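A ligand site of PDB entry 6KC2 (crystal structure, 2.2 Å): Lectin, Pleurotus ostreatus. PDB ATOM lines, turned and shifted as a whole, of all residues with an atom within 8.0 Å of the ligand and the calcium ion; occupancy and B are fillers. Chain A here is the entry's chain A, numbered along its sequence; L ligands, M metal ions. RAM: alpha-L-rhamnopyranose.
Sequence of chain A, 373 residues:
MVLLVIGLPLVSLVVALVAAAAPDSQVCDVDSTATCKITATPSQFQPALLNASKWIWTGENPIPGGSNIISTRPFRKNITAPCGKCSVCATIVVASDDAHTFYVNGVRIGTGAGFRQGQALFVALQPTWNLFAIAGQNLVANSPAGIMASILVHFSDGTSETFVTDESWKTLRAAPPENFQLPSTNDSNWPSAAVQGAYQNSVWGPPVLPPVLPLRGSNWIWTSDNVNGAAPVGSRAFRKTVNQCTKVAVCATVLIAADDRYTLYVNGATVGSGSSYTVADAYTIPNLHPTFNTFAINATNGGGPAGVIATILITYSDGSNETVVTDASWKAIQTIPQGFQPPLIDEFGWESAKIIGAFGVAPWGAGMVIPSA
The backbone carbonyl oxygen of Asn 68 sits at hydrogen-bond distance from the side-chain amide nitrogen of Asn 138 (3.1 Å). The side-chain amide nitrogen (ND2) of Asn 138 sits at hydrogen-bond distance from the backbone carbonyl oxygen (O) of Ile 69 (3.0 Å). The side-chain carboxylate of Asp 98 sits close to the backbone NH of Leu 139, 2.7 Å away. The backbone NH of Asp 98 is in hydrogen-bond range of the backbone carbonyl oxygen of Gln 137. The backbone NH (N) of Gly 114 lies within hydrogen-bond range of the backbone carbonyl oxygen (O) of Asp 98 (3.1 Å). O of Val 140 sits close to OG of Ser 143 (2.6 Å). The backbone carbonyl oxygen of Ser 143 is in hydrogen-bond range of the backbone NH of Asn 68 (2.9 Å). O of Ser 96 sits at hydrogen-bond distance from N of Phe 115.
Merely in contact with the ligand: Phe 115 and Val 140. Hydrophobic or aromatic side chains that line the ligand: Phe 115, Val 140 and Pro 144. Within 4 Å of the ligand: Asp 97, Asp 98, Phe 115, Val 140, Ser 143 and Pro 144. The nearest printed residue that does not touch the ligand is Asn 138 (4.2 Å).
Of the 26 residues printed, 5 come within 4 Å of the calcium ion. Along chain A the residues within 4 Å of the calcium ion span positions 97 to 144.
The calcium ion is bound by the side-chain amide oxygen of Asn 138, the side-chain carboxylate of Asp 97, the backbone carbonyl oxygen of Pro 144, an oxygen (O4) of the ligand, an oxygen (O3) of the ligand, the side-chain hydroxyl of Ser 143 and the side-chain carboxylate of Asp 98. The calcium ion has seven donor atoms within binding distance.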
ATOM      1  N   TRP A  57       1.487  18.369  26.400  1.00  0.00           N
ATOM      2  CA  TRP A  57       0.846  18.270  27.697  1.00  0.00           C
ATOM      3  C   TRP A  57       1.873  18.738  28.711  1.00  0.00           C
ATOM      4  O   TRP A  57       2.818  19.463  28.361  1.00  0.00           O
ATOM      5  CB  TRP A  57       0.327  16.842  27.947  1.00  0.00           C
ATOM      6  CG  TRP A  57      -0.700  16.784  29.050  1.00  0.00           C
ATOM      7  CD1 TRP A  57      -0.587  16.118  30.238  1.00  0.00           C
ATOM      8  CD2 TRP A  57      -1.985  17.431  29.070  1.00  0.00           C
ATOM      9  NE1 TRP A  57      -1.718  16.302  30.986  1.00  0.00           N
ATOM     10  CE2 TRP A  57      -2.592  17.107  30.303  1.00  0.00           C
ATOM     11  CE3 TRP A  57      -2.677  18.260  28.169  1.00  0.00           C
ATOM     12  CZ2 TRP A  57      -3.870  17.569  30.668  1.00  0.00           C
ATOM     13  CZ3 TRP A  57      -3.954  18.726  28.526  1.00  0.00           C
ATOM     14  CH2 TRP A  57      -4.538  18.375  29.767  1.00  0.00           C
ATOM     15  N   GLY A  65       2.159  10.292  25.300  1.00  0.00           N
ATOM     16  CA  GLY A  65       1.023   9.457  24.981  1.00  0.00           C
ATOM     17  C   GLY A  65       0.653   8.494  26.089  1.00  0.00           C
ATOM     18  O   GLY A  65      -0.148   7.580  25.867  1.00  0.00           O
ATOM     19  N   GLY A  66       1.221   8.682  27.271  1.00  0.00           N
ATOM     20  CA  GLY A  66       0.952   7.815  28.388  1.00  0.00           C
ATOM     21  C   GLY A  66      -0.312   8.216  29.129  1.00  0.00           C
ATOM     22  O   GLY A  66      -0.952   9.230  28.850  1.00  0.00           O
ATOM     23  N   SER A  67      -0.658   7.393  30.114  1.00  0.00           N
ATOM     24  CA  SER A  67      -1.860   7.641  30.896  1.00  0.00           C
ATOM     25  C   SER A  67      -1.665   8.873  31.779  1.00  0.00           C
ATOM     26  O   SER A  67      -0.586   9.092  32.353  1.00  0.00           O
ATOM     27  CB  SER A  67      -2.218   6.407  31.723  1.00  0.00           C
ATOM     28  OG  SER A  67      -1.663   6.480  32.998  1.00  0.00           O
ATOM     29  N   ASN A  68      -2.706   9.690  31.865  1.00  0.00           N
ATOM     30  CA  ASN A  68      -2.722  10.903  32.673  1.00  0.00           C
ATOM     31  C   ASN A  68      -4.005  10.940  33.484  1.00  0.00           C
ATOM     32  O   ASN A  68      -5.002  10.275  33.163  1.00  0.00           O
ATOM     33  CB  ASN A  68      -2.625  12.148  31.797  1.00  0.00           C
ATOM     34  CG  ASN A  68      -1.196  12.373  31.298  1.00  0.00           C
ATOM     35  OD1 ASN A  68      -0.769  11.792  30.286  1.00  0.00           O
ATOM     36  ND2 ASN A  68      -0.461  13.198  32.013  1.00  0.00           N
ATOM     37  N   ILE A  69      -3.971  11.726  34.542  1.00  0.00           N
ATOM     38  CA  ILE A  69      -5.129  11.883  35.424  1.00  0.00           C
ATOM     39  C   ILE A  69      -6.118  12.873  34.821  1.00  0.00           C
ATOM     40  O   ILE A  69      -5.765  13.723  33.994  1.00  0.00           O
ATOM     41  CB  ILE A  69      -4.678  12.342  36.820  1.00  0.00           C
ATOM     42  CG1 ILE A  69      -4.109  13.769  36.714  1.00  0.00           C
ATOM     43  CG2 ILE A  69      -3.619  11.373  37.430  1.00  0.00           C
ATOM     44  CD1 ILE A  69      -4.002  14.483  38.074  1.00  0.00           C
ATOM     45  N   ILE A  70      -7.369  12.778  35.272  1.00  0.00           N
ATOM     46  CA  ILE A  70      -8.349  13.829  34.988  1.00  0.00           C
ATOM     47  C   ILE A  70      -7.835  15.132  35.577  1.00  0.00           C
ATOM     48  O   ILE A  70      -7.439  15.197  36.752  1.00  0.00           O
ATOM     49  CB  ILE A  70      -9.723  13.448  35.549  1.00  0.00           C
ATOM     50  CG1 ILE A  70     -10.247  12.193  34.835  1.00  0.00           C
ATOM     51  CG2 ILE A  70     -10.697  14.600  35.362  1.00  0.00           C
ATOM     52  CD1 ILE A  70     -11.549  11.638  35.413  1.00  0.00           C
ATOM     53  N   SER A  96      -7.752  18.458  20.414  1.00  0.00           N
ATOM     54  CA  SER A  96      -7.467  18.196  21.815  1.00  0.00           C
ATOM     55  C   SER A  96      -7.911  16.804  22.222  1.00  0.00           C
ATOM     56  O   SER A  96      -8.894  16.249  21.721  1.00  0.00           O
ATOM     57  CB  SER A  96      -8.153  19.201  22.747  1.00  0.00           C
ATOM     58  OG  SER A  96      -9.551  19.267  22.487  1.00  0.00           O
ATOM     59  N   ASP A  97      -7.186  16.275  23.190  1.00  0.00           N
ATOM     60  CA  ASP A  97      -7.601  15.095  23.940  1.00  0.00           C
ATOM     61  C   ASP A  97      -7.543  15.531  25.396  1.00  0.00           C
ATOM     62  O   ASP A  97      -6.444  15.580  25.961  1.00  0.00           O
ATOM     63  CB  ASP A  97      -6.664  13.925  23.643  1.00  0.00           C
ATOM     64  CG  ASP A  97      -6.977  12.694  24.476  1.00  0.00           C
ATOM     65  OD1 ASP A  97      -7.808  12.777  25.410  1.00  0.00           O
ATOM     66  OD2 ASP A  97      -6.384  11.639  24.174  1.00  0.00           O
ATOM     67  N   ASP A  98      -8.697  15.840  26.008  1.00  0.00           N
ATOM     68  CA  ASP A  98     -10.046  15.644  25.451  1.00  0.00           C
ATOM     69  C   ASP A  98     -10.766  16.929  24.990  1.00  0.00           C
ATOM     70  O   ASP A  98     -11.637  16.870  24.132  1.00  0.00           O
ATOM     71  CB  ASP A  98     -10.966  14.967  26.490  1.00  0.00           C
ATOM     72  CG  ASP A  98     -10.505  13.578  26.866  1.00  0.00           C
ATOM     73  OD1 ASP A  98     -10.947  12.622  26.189  1.00  0.00           O
ATOM     74  OD2 ASP A  98      -9.743  13.440  27.865  1.00  0.00           O
ATOM     75  N   ALA A  99     -10.444  18.079  25.600  1.00  0.00           N
ATOM     76  CA  ALA A  99     -11.204  19.299  25.354  1.00  0.00           C
ATOM     77  C   ALA A  99     -10.304  20.513  25.533  1.00  0.00           C
ATOM     78  O   ALA A  99      -9.269  20.436  26.216  1.00  0.00           O
ATOM     79  CB  ALA A  99     -12.437  19.398  26.290  1.00  0.00           C
ATOM     80  N   GLY A 114     -11.847  16.961  21.048  1.00  0.00           N
ATOM     81  CA  GLY A 114     -11.707  15.844  20.132  1.00  0.00           C
ATOM     82  C   GLY A 114     -10.431  15.944  19.310  1.00  0.00           C
ATOM     83  O   GLY A 114      -9.991  17.043  18.936  1.00  0.00           O
ATOM     84  N   PHE A 115      -9.851  14.798  19.010  1.00  0.00           N
ATOM     85  CA  PHE A 115      -8.567  14.739  18.315  1.00  0.00           C
ATOM     86  C   PHE A 115      -8.668  14.157  16.919  1.00  0.00           C
ATOM     87  O   PHE A 115      -7.686  14.224  16.159  1.00  0.00           O
ATOM     88  CB  PHE A 115      -7.559  13.913  19.138  1.00  0.00           C
ATOM     89  CG  PHE A 115      -8.014  12.503  19.416  1.00  0.00           C
ATOM     90  CD1 PHE A 115      -7.731  11.474  18.506  1.00  0.00           C
ATOM     91  CD2 PHE A 115      -8.722  12.197  20.580  1.00  0.00           C
ATOM     92  CE1 PHE A 115      -8.144  10.161  18.764  1.00  0.00           C
ATOM     93  CE2 PHE A 115      -9.155  10.894  20.843  1.00  0.00           C
ATOM     94  CZ  PHE A 115      -8.868   9.882  19.932  1.00  0.00           C
ATOM     95  N   ARG A 116      -9.822  13.582  16.546  1.00  0.00           N
ATOM     96  CA  ARG A 116      -9.968  13.009  15.222  1.00  0.00           C
ATOM     97  C   ARG A 116     -10.137  14.080  14.159  1.00  0.00           C
ATOM     98  O   ARG A 116      -9.742  13.880  13.001  1.00  0.00           O
ATOM     99  CB  ARG A 116     -11.161  12.039  15.192  1.00  0.00           C
ATOM    100  CG  ARG A 116     -11.055  10.864  16.187  1.00  0.00           C
ATOM    101  CD  ARG A 116     -10.500   9.593  15.539  1.00  0.00           C
ATOM    102  NE  ARG A 116     -10.461   8.453  16.479  1.00  0.00           N
ATOM    103  CZ  ARG A 116      -9.416   7.633  16.627  1.00  0.00           C
ATOM    104  NH1 ARG A 116      -8.322   7.803  15.903  1.00  0.00           N
ATOM    105  NH2 ARG A 116      -9.479   6.635  17.516  1.00  0.00           N
ATOM    106  N   GLN A 137      -8.080  19.971  28.822  1.00  0.00           N
ATOM    107  CA  GLN A 137      -8.669  19.121  29.853  1.00  0.00           C
ATOM    108  C   GLN A 137      -8.563  17.661  29.441  1.00  0.00           C
ATOM    109  O   GLN A 137      -8.963  17.299  28.331  1.00  0.00           O
ATOM    110  CB  GLN A 137     -10.155  19.424  30.105  1.00  0.00           C
ATOM    111  CG  GLN A 137     -10.542  20.859  30.385  1.00  0.00           C
ATOM    112  CD  GLN A 137     -12.075  21.016  30.346  1.00  0.00           C
ATOM    113  OE1 GLN A 137     -12.796  20.277  31.022  1.00  0.00           O
ATOM    114  NE2 GLN A 137     -12.566  21.954  29.516  1.00  0.00           N
ATOM    115  N   ASN A 138      -8.052  16.830  30.350  1.00  0.00           N
ATOM    116  CA  ASN A 138      -8.158  15.389  30.238  1.00  0.00           C
ATOM    117  C   ASN A 138      -9.411  14.943  31.003  1.00  0.00           C
ATOM    118  O   ASN A 138      -9.531  15.228  32.200  1.00  0.00           O
ATOM    119  CB  ASN A 138      -6.914  14.713  30.783  1.00  0.00           C
ATOM    120  CG  ASN A 138      -6.892  13.238  30.484  1.00  0.00           C
ATOM    121  OD1 ASN A 138      -7.521  12.788  29.525  1.00  0.00           O
ATOM    122  ND2 ASN A 138      -6.157  12.464  31.293  1.00  0.00           N
ATOM    123  N   LEU A 139     -10.325  14.248  30.330  1.00  0.00           N
ATOM    124  CA  LEU A 139     -11.622  13.942  30.930  1.00  0.00           C
ATOM    125  C   LEU A 139     -11.813  12.467  31.260  1.00  0.00           C
ATOM    126  O   LEU A 139     -12.831  12.112  31.853  1.00  0.00           O
ATOM    127  CB  LEU A 139     -12.766  14.430  30.020  1.00  0.00           C
ATOM    128  CG  LEU A 139     -12.855  15.952  29.825  1.00  0.00           C
ATOM    129  CD1 LEU A 139     -13.915  16.330  28.784  1.00  0.00           C
ATOM    130  CD2 LEU A 139     -13.150  16.662  31.150  1.00  0.00           C
ATOM    131  N   VAL A 140     -10.871  11.598  30.889  1.00  0.00           N
ATOM    132  CA  VAL A 140     -10.974  10.172  31.173  1.00  0.00           C
ATOM    133  C   VAL A 140      -9.734   9.755  31.959  1.00  0.00           C
ATOM    134  O   VAL A 140      -8.607  10.064  31.545  1.00  0.00           O
ATOM    135  CB  VAL A 140     -11.123   9.347  29.883  1.00  0.00           C
ATOM    136  CG1 VAL A 140     -11.171   7.868  30.187  1.00  0.00           C
ATOM    137  CG2 VAL A 140     -12.360   9.771  29.138  1.00  0.00           C
ATOM    138  N   ALA A 141      -9.933   9.070  33.086  1.00  0.00           N
ATOM    139  CA  ALA A 141      -8.802   8.674  33.910  1.00  0.00           C
ATOM    140  C   ALA A 141      -7.937   7.639  33.197  1.00  0.00           C
ATOM    141  O   ALA A 141      -8.428   6.855  32.386  1.00  0.00           O
ATOM    142  CB  ALA A 141      -9.287   8.119  35.258  1.00  0.00           C
ATOM    143  N   ASN A 142      -6.627   7.653  33.488  1.00  0.00           N
ATOM    144  CA  ASN A 142      -5.668   6.715  32.923  1.00  0.00           C
ATOM    145  C   ASN A 142      -5.563   6.802  31.399  1.00  0.00           C
ATOM    146  O   ASN A 142      -5.199   5.814  30.745  1.00  0.00           O
ATOM    147  CB  ASN A 142      -5.997   5.260  33.301  1.00  0.00           C
ATOM    148  CG  ASN A 142      -6.116   5.050  34.783  1.00  0.00           C
ATOM    149  OD1 ASN A 142      -5.262   5.485  35.552  1.00  0.00           O
ATOM    150  ND2 ASN A 142      -7.200   4.406  35.195  1.00  0.00           N
ATOM    151  N   SER A 143      -5.886   7.945  30.814  1.00  0.00           N
ATOM    152  CA  SER A 143      -5.942   8.077  29.364  1.00  0.00           C
ATOM    153  C   SER A 143      -4.957   9.141  28.894  1.00  0.00           C
ATOM    154  O   SER A 143      -4.538  10.002  29.665  1.00  0.00           O
ATOM    155  CB  SER A 143      -7.365   8.443  28.896  1.00  0.00           C
ATOM    156  OG  SER A 143      -7.639   9.799  29.173  1.00  0.00           O
ATOM    157  N   PRO A 144      -4.568   9.112  27.617  1.00  0.00           N
ATOM    158  CA  PRO A 144      -3.658  10.141  27.109  1.00  0.00           C
ATOM    159  C   PRO A 144      -4.276  11.530  27.189  1.00  0.00           C
ATOM    160  O   PRO A 144      -5.485  11.695  27.345  1.00  0.00           O
ATOM    161  CB  PRO A 144      -3.383   9.734  25.650  1.00  0.00           C
ATOM    162  CG  PRO A 144      -4.148   8.492  25.406  1.00  0.00           C
ATOM    163  CD  PRO A 144      -4.709   7.967  26.696  1.00  0.00           C
ATOM    164  N   ALA A 145      -3.422  12.534  27.096  1.00  0.00           N
ATOM    165  CA  ALA A 145      -3.861  13.918  27.152  1.00  0.00           C
ATOM    166  C   ALA A 145      -2.957  14.750  26.254  1.00  0.00           C
ATOM    167  O   ALA A 145      -1.739  14.531  26.207  1.00  0.00           O
ATOM    168  CB  ALA A 145      -3.847  14.456  28.585  1.00  0.00           C
ATOM    169  N   GLY A 146      -3.542  15.718  25.564  1.00  0.00           N
ATOM    170  CA  GLY A 146      -2.772  16.512  24.631  1.00  0.00           C
ATOM    171  C   GLY A 146      -3.519  17.608  23.912  1.00  0.00           C
ATOM    172  O   GLY A 146      -4.734  17.512  23.673  1.00  0.00           O
ATOM    173  N   VAL A 203       0.027   8.731  19.492  1.00  0.00           N
ATOM    174  CA  VAL A 203      -1.043   7.787  19.781  1.00  0.00           C
ATOM    175  C   VAL A 203      -2.335   8.183  19.061  1.00  0.00           C
ATOM    176  O   VAL A 203      -3.177   7.323  18.785  1.00  0.00           O
ATOM    177  CB  VAL A 203      -1.278   7.638  21.291  1.00  0.00           C
ATOM    178  CG1 VAL A 203      -0.078   6.972  21.933  1.00  0.00           C
ATOM    179  CG2 VAL A 203      -1.605   8.991  21.949  1.00  0.00           C
ATOM    180  N   TRP A 204      -2.477   9.469  18.706  1.00  0.00           N
ATOM    181  CA  TRP A 204      -3.729   9.949  18.135  1.00  0.00           C
ATOM    182  C   TRP A 204      -3.839   9.747  16.629  1.00  0.00           C
ATOM    183  O   TRP A 204      -4.952   9.657  16.120  1.00  0.00           O
ATOM    184  CB  TRP A 204      -3.914  11.428  18.481  1.00  0.00           C
ATOM    185  CG  TRP A 204      -4.015  11.603  19.953  1.00  0.00           C
ATOM    186  CD1 TRP A 204      -5.105  11.296  20.758  1.00  0.00           C
ATOM    187  CD2 TRP A 204      -2.981  12.067  20.836  1.00  0.00           C
ATOM    188  NE1 TRP A 204      -4.796  11.556  22.080  1.00  0.00           N
ATOM    189  CE2 TRP A 204      -3.511  12.040  22.150  1.00  0.00           C
ATOM    190  CE3 TRP A 204      -1.667  12.520  20.632  1.00  0.00           C
ATOM    191  CZ2 TRP A 204      -2.762  12.444  23.256  1.00  0.00           C
ATOM    192  CZ3 TRP A 204      -0.934  12.916  21.730  1.00  0.00           C
ATOM    193  CH2 TRP A 204      -1.480  12.886  23.030  1.00  0.00           C
HETATM  194  C1  RAM L   1     -10.784   7.515  24.908  1.00  0.00           C
HETATM  195  C2  RAM L   1     -11.072   8.828  25.639  1.00  0.00           C
HETATM  196  C3  RAM L   1      -9.778   9.309  26.295  1.00  0.00           C
HETATM  197  C4  RAM L   1      -8.721   9.498  25.216  1.00  0.00           C
HETATM  198  C5  RAM L   1      -8.568   8.219  24.390  1.00  0.00           C
HETATM  199  C6  RAM L   1      -7.628   8.428  23.219  1.00  0.00           C
HETATM  200  O1  RAM L   1     -10.347   6.507  25.844  1.00  0.00           O
HETATM  201  O2  RAM L   1     -11.494   9.804  24.708  1.00  0.00           O
HETATM  202  O3  RAM L   1     -10.027  10.522  26.967  1.00  0.00           O
HETATM  203  O4  RAM L   1      -7.512   9.871  25.834  1.00  0.00           O
HETATM  204  O5  RAM L   1      -9.823   7.781  23.881  1.00  0.00           O
HETATM  205 CA    CA M   1      -7.892  11.659  27.504  1.00  0.00          CA
